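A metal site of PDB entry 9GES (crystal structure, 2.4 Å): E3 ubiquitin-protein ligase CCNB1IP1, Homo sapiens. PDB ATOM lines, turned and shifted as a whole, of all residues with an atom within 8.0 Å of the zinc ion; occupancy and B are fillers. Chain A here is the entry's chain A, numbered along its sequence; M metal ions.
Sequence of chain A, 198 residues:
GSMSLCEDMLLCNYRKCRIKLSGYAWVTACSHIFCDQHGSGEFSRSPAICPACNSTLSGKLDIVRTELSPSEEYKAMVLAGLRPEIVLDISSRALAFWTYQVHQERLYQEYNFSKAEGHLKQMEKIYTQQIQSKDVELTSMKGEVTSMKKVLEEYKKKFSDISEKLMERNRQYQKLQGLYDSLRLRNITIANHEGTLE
The zinc ion is bound by ND1 of His 32 (2.0 Å), SG of Cys 30 (2.3 Å), SG of Cys 50 (2.3 Å) and SG of Cys 53 (2.3 Å). The zinc ion has four donor atoms within binding distance.
Thr 28 touches the zinc ion. Along chain A the residues within 4 Å of the zinc ion span positions 28 to 53. The nearest printed residue that does not touch the zinc ion is Ala 52 (4.5 Å).
The backbone NH (N) of His 32 lies within hydrogen-bond range of the side-chain hydroxyl (OG1) of Thr 28 (3.0 Å). The side-chain hydroxyl (OG) of Ser 55 lies close to the side-chain sulfur (SG) of Cys 53 (3.0 Å). O of Ser 55 lies within hydrogen-bond range of N of Cys 50 (3.2 Å). The side-chain sulfur of Cys 50 sits close to the backbone NH of Ala 52. OG1 of Thr 28 sits close to N of Cys 30 (3.4 Å).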
ATOM      1  N   ASN A  13      -8.127  19.242 -13.461  1.00  0.00           N
ATOM      2  CA  ASN A  13      -8.595  20.455 -12.812  1.00  0.00           C
ATOM      3  C   ASN A  13      -7.928  21.711 -13.357  1.00  0.00           C
ATOM      4  O   ASN A  13      -8.271  22.810 -12.913  1.00  0.00           O
ATOM      5  CB  ASN A  13      -8.395  20.362 -11.297  1.00  0.00           C
ATOM      6  CG  ASN A  13      -9.344  19.386 -10.628  1.00  0.00           C
ATOM      7  OD1 ASN A  13      -8.957  18.601  -9.765  1.00  0.00           O
ATOM      8  ND2 ASN A  13     -10.610  19.426 -11.043  1.00  0.00           N
ATOM      9  N   THR A  28      -3.876  16.587  -5.067  1.00  0.00           N
ATOM     10  CA  THR A  28      -3.443  17.599  -4.122  1.00  0.00           C
ATOM     11  C   THR A  28      -4.217  17.479  -2.808  1.00  0.00           C
ATOM     12  O   THR A  28      -5.327  16.946  -2.770  1.00  0.00           O
ATOM     13  CB  THR A  28      -3.614  19.007  -4.692  1.00  0.00           C
ATOM     14  OG1 THR A  28      -5.009  19.348  -4.717  1.00  0.00           O
ATOM     15  CG2 THR A  28      -3.063  19.082  -6.103  1.00  0.00           C
ATOM     16  N   ALA A  29      -3.601  17.989  -1.736  1.00  0.00           N
ATOM     17  CA  ALA A  29      -4.262  18.027  -0.442  1.00  0.00           C
ATOM     18  C   ALA A  29      -5.464  18.966  -0.427  1.00  0.00           C
ATOM     19  O   ALA A  29      -6.314  18.842   0.458  1.00  0.00           O
ATOM     20  CB  ALA A  29      -3.268  18.433   0.646  1.00  0.00           C
ATOM     21  N   CYS A  30      -5.530  19.905  -1.363  1.00  0.00           N
ATOM     22  CA  CYS A  30      -6.665  20.814  -1.490  1.00  0.00           C
ATOM     23  C   CYS A  30      -7.788  20.232  -2.346  1.00  0.00           C
ATOM     24  O   CYS A  30      -8.592  20.991  -2.893  1.00  0.00           O
ATOM     25  CB  CYS A  30      -6.197  22.157  -2.055  1.00  0.00           C
ATOM     26  SG  CYS A  30      -5.140  22.021  -3.512  1.00  0.00           S
ATOM     27  N   SER A  31      -7.836  18.902  -2.485  1.00  0.00           N
ATOM     28  CA  SER A  31      -8.920  18.202  -3.180  1.00  0.00           C
ATOM     29  C   SER A  31      -8.973  18.602  -4.664  1.00  0.00           C
ATOM     30  O   SER A  31     -10.024  18.989  -5.179  1.00  0.00           O
ATOM     31  CB  SER A  31     -10.265  18.439  -2.485  1.00  0.00           C
ATOM     32  OG  SER A  31     -10.226  17.949  -1.158  1.00  0.00           O
ATOM     33  N   HIS A  32      -7.835  18.486  -5.331  1.00  0.00           N
ATOM     34  CA  HIS A  32      -7.761  18.705  -6.772  1.00  0.00           C
ATOM     35  C   HIS A  32      -6.891  17.622  -7.392  1.00  0.00           C
ATOM     36  O   HIS A  32      -6.012  17.052  -6.738  1.00  0.00           O
ATOM     37  CB  HIS A  32      -7.200  20.092  -7.124  1.00  0.00           C
ATOM     38  CG  HIS A  32      -8.133  21.211  -6.778  1.00  0.00           C
ATOM     39  ND1 HIS A  32      -7.882  22.092  -5.744  1.00  0.00           N
ATOM     40  CD2 HIS A  32      -9.314  21.583  -7.315  1.00  0.00           C
ATOM     41  CE1 HIS A  32      -8.874  22.969  -5.677  1.00  0.00           C
ATOM     42  NE2 HIS A  32      -9.753  22.687  -6.612  1.00  0.00           N
ATOM     43  N   ILE A  33      -7.134  17.351  -8.675  1.00  0.00           N
ATOM     44  CA  ILE A  33      -6.425  16.310  -9.408  1.00  0.00           C
ATOM     45  C   ILE A  33      -6.145  16.807 -10.823  1.00  0.00           C
ATOM     46  O   ILE A  33      -6.992  17.464 -11.442  1.00  0.00           O
ATOM     47  CB  ILE A  33      -7.210  14.983  -9.416  1.00  0.00           C
ATOM     48  CG1 ILE A  33      -6.371  13.857 -10.027  1.00  0.00           C
ATOM     49  CG2 ILE A  33      -8.548  15.142 -10.128  1.00  0.00           C
ATOM     50  CD1 ILE A  33      -7.015  12.492  -9.900  1.00  0.00           C
ATOM     51  N   PHE A  34      -4.958  16.509 -11.333  1.00  0.00           N
ATOM     52  CA  PHE A  34      -4.517  17.005 -12.628  1.00  0.00           C
ATOM     53  C   PHE A  34      -3.921  15.858 -13.441  1.00  0.00           C
ATOM     54  O   PHE A  34      -3.523  14.822 -12.903  1.00  0.00           O
ATOM     55  CB  PHE A  34      -3.473  18.126 -12.476  1.00  0.00           C
ATOM     56  CG  PHE A  34      -3.969  19.302 -11.675  1.00  0.00           C
ATOM     57  CD1 PHE A  34      -3.809  19.339 -10.305  1.00  0.00           C
ATOM     58  CD2 PHE A  34      -4.598  20.362 -12.299  1.00  0.00           C
ATOM     59  CE1 PHE A  34      -4.268  20.409  -9.563  1.00  0.00           C
ATOM     60  CE2 PHE A  34      -5.057  21.448 -11.570  1.00  0.00           C
ATOM     61  CZ  PHE A  34      -4.897  21.472 -10.202  1.00  0.00           C
ATOM     62  N   PHE A  43       3.824  20.566 -10.505  1.00  0.00           N
ATOM     63  CA  PHE A  43       4.144  20.083  -9.166  1.00  0.00           C
ATOM     64  C   PHE A  43       5.534  19.479  -9.060  1.00  0.00           C
ATOM     65  O   PHE A  43       5.792  18.677  -8.155  1.00  0.00           O
ATOM     66  CB  PHE A  43       3.082  19.096  -8.697  1.00  0.00           C
ATOM     67  CG  PHE A  43       1.725  19.701  -8.531  1.00  0.00           C
ATOM     68  CD1 PHE A  43       1.395  20.382  -7.371  1.00  0.00           C
ATOM     69  CD2 PHE A  43       0.768  19.587  -9.525  1.00  0.00           C
ATOM     70  CE1 PHE A  43       0.148  20.943  -7.214  1.00  0.00           C
ATOM     71  CE2 PHE A  43      -0.479  20.150  -9.381  1.00  0.00           C
ATOM     72  CZ  PHE A  43      -0.799  20.837  -8.214  1.00  0.00           C
ATOM     73  N   ILE A  49       2.219  25.886  -6.796  1.00  0.00           N
ATOM     74  CA  ILE A  49       0.924  26.538  -6.617  1.00  0.00           C
ATOM     75  C   ILE A  49      -0.113  25.725  -7.380  1.00  0.00           C
ATOM     76  O   ILE A  49       0.084  25.401  -8.562  1.00  0.00           O
ATOM     77  CB  ILE A  49       0.944  27.986  -7.110  1.00  0.00           C
ATOM     78  CG1 ILE A  49       1.913  28.832  -6.269  1.00  0.00           C
ATOM     79  CG2 ILE A  49      -0.454  28.591  -7.080  1.00  0.00           C
ATOM     80  CD1 ILE A  49       1.526  28.939  -4.811  1.00  0.00           C
ATOM     81  N   CYS A  50      -1.201  25.381  -6.712  1.00  0.00           N
ATOM     82  CA  CYS A  50      -2.275  24.622  -7.353  1.00  0.00           C
ATOM     83  C   CYS A  50      -2.924  25.465  -8.425  1.00  0.00           C
ATOM     84  O   CYS A  50      -3.439  26.547  -8.125  1.00  0.00           O
ATOM     85  CB  CYS A  50      -3.299  24.172  -6.322  1.00  0.00           C
ATOM     86  SG  CYS A  50      -4.707  23.255  -7.012  1.00  0.00           S
ATOM     87  N   PRO A  51      -2.941  25.022  -9.687  1.00  0.00           N
ATOM     88  CA  PRO A  51      -3.520  25.856 -10.755  1.00  0.00           C
ATOM     89  C   PRO A  51      -5.003  26.141 -10.587  1.00  0.00           C
ATOM     90  O   PRO A  51      -5.513  27.095 -11.186  1.00  0.00           O
ATOM     91  CB  PRO A  51      -3.244  25.051 -12.033  1.00  0.00           C
ATOM     92  CG  PRO A  51      -2.085  24.171 -11.680  1.00  0.00           C
ATOM     93  CD  PRO A  51      -2.271  23.824 -10.229  1.00  0.00           C
ATOM     94  N   ALA A  52      -5.717  25.327  -9.795  1.00  0.00           N
ATOM     95  CA  ALA A  52      -7.162  25.509  -9.665  1.00  0.00           C
ATOM     96  C   ALA A  52      -7.497  26.590  -8.637  1.00  0.00           C
ATOM     97  O   ALA A  52      -8.153  27.584  -8.964  1.00  0.00           O
ATOM     98  CB  ALA A  52      -7.812  24.176  -9.275  1.00  0.00           C
ATOM     99  N   CYS A  53      -7.062  26.411  -7.389  1.00  0.00           N
ATOM    100  CA  CYS A  53      -7.419  27.304  -6.296  1.00  0.00           C
ATOM    101  C   CYS A  53      -6.275  28.187  -5.824  1.00  0.00           C
ATOM    102  O   CYS A  53      -6.457  28.931  -4.863  1.00  0.00           O
ATOM    103  CB  CYS A  53      -7.958  26.484  -5.121  1.00  0.00           C
ATOM    104  SG  CYS A  53      -6.803  25.254  -4.485  1.00  0.00           S
ATOM    105  N   ASN A  54      -5.116  28.103  -6.465  1.00  0.00           N
ATOM    106  CA  ASN A  54      -3.935  28.919  -6.117  1.00  0.00           C
ATOM    107  C   ASN A  54      -3.478  28.704  -4.682  1.00  0.00           C
ATOM    108  O   ASN A  54      -2.813  29.568  -4.107  1.00  0.00           O
ATOM    109  CB  ASN A  54      -4.190  30.403  -6.381  1.00  0.00           C
ATOM    110  CG  ASN A  54      -4.275  30.731  -7.861  1.00  0.00           C
ATOM    111  OD1 ASN A  54      -3.589  30.112  -8.679  1.00  0.00           O
ATOM    112  ND2 ASN A  54      -5.102  31.705  -8.217  1.00  0.00           N
ATOM    113  N   SER A  55      -3.812  27.560  -4.081  1.00  0.00           N
ATOM    114  CA  SER A  55      -3.358  27.266  -2.736  1.00  0.00           C
ATOM    115  C   SER A  55      -1.864  26.949  -2.744  1.00  0.00           C
ATOM    116  O   SER A  55      -1.349  26.323  -3.676  1.00  0.00           O
ATOM    117  CB  SER A  55      -4.132  26.085  -2.157  1.00  0.00           C
ATOM    118  OG  SER A  55      -5.504  26.406  -2.006  1.00  0.00           O
ATOM    119  N   THR A  56      -1.170  27.382  -1.692  1.00  0.00           N
ATOM    120  CA  THR A  56       0.268  27.167  -1.562  1.00  0.00           C
ATOM    121  C   THR A  56       0.502  25.809  -0.907  1.00  0.00           C
ATOM    122  O   THR A  56       0.306  25.657   0.302  1.00  0.00           O
ATOM    123  CB  THR A  56       0.911  28.299  -0.774  1.00  0.00           C
ATOM    124  OG1 THR A  56       0.745  29.539  -1.469  1.00  0.00           O
ATOM    125  CG2 THR A  56       2.409  28.030  -0.582  1.00  0.00           C
ATOM    126  N   LEU A  57       0.902  24.835  -1.705  1.00  0.00           N
ATOM    127  CA  LEU A  57       1.213  23.502  -1.218  1.00  0.00           C
ATOM    128  C   LEU A  57       2.713  23.358  -1.043  1.00  0.00           C
ATOM    129  O   LEU A  57       3.486  23.654  -1.965  1.00  0.00           O
ATOM    130  CB  LEU A  57       0.689  22.438  -2.184  1.00  0.00           C
ATOM    131  CG  LEU A  57      -0.805  22.508  -2.528  1.00  0.00           C
ATOM    132  CD1 LEU A  57      -1.150  21.493  -3.610  1.00  0.00           C
ATOM    133  CD2 LEU A  57      -1.652  22.272  -1.288  1.00  0.00           C
ATOM    134  N   TYR A 100     -16.489  15.823  -3.973  1.00  0.00           N
ATOM    135  CA  TYR A 100     -16.096  17.197  -4.261  1.00  0.00           C
ATOM    136  C   TYR A 100     -15.844  17.399  -5.757  1.00  0.00           C
ATOM    137  O   TYR A 100     -16.263  18.405  -6.335  1.00  0.00           O
ATOM    138  CB  TYR A 100     -14.857  17.583  -3.450  1.00  0.00           C
ATOM    139  CG  TYR A 100     -14.354  18.977  -3.743  1.00  0.00           C
ATOM    140  CD1 TYR A 100     -14.935  20.084  -3.138  1.00  0.00           C
ATOM    141  CD2 TYR A 100     -13.303  19.189  -4.624  1.00  0.00           C
ATOM    142  CE1 TYR A 100     -14.484  21.366  -3.397  1.00  0.00           C
ATOM    143  CE2 TYR A 100     -12.842  20.465  -4.892  1.00  0.00           C
ATOM    144  CZ  TYR A 100     -13.433  21.543  -4.277  1.00  0.00           C
ATOM    145  OH  TYR A 100     -12.982  22.819  -4.544  1.00  0.00           O
ATOM    146  N   GLN A 101     -15.161  16.436  -6.384  1.00  0.00           N
ATOM    147  CA  GLN A 101     -14.910  16.529  -7.825  1.00  0.00           C
ATOM    148  C   GLN A 101     -16.213  16.484  -8.611  1.00  0.00           C
ATOM    149  O   GLN A 101     -16.373  17.217  -9.591  1.00  0.00           O
ATOM    150  CB  GLN A 101     -13.968  15.409  -8.258  1.00  0.00           C
ATOM    151  CG  GLN A 101     -12.518  15.637  -7.896  1.00  0.00           C
ATOM    152  CD  GLN A 101     -11.887  16.761  -8.690  1.00  0.00           C
ATOM    153  OE1 GLN A 101     -12.327  17.068  -9.796  1.00  0.00           O
ATOM    154  NE2 GLN A 101     -10.847  17.370  -8.136  1.00  0.00           N
HETATM  155 ZN    ZN M   1      -6.194  23.115  -5.228  1.00  0.00          ZN
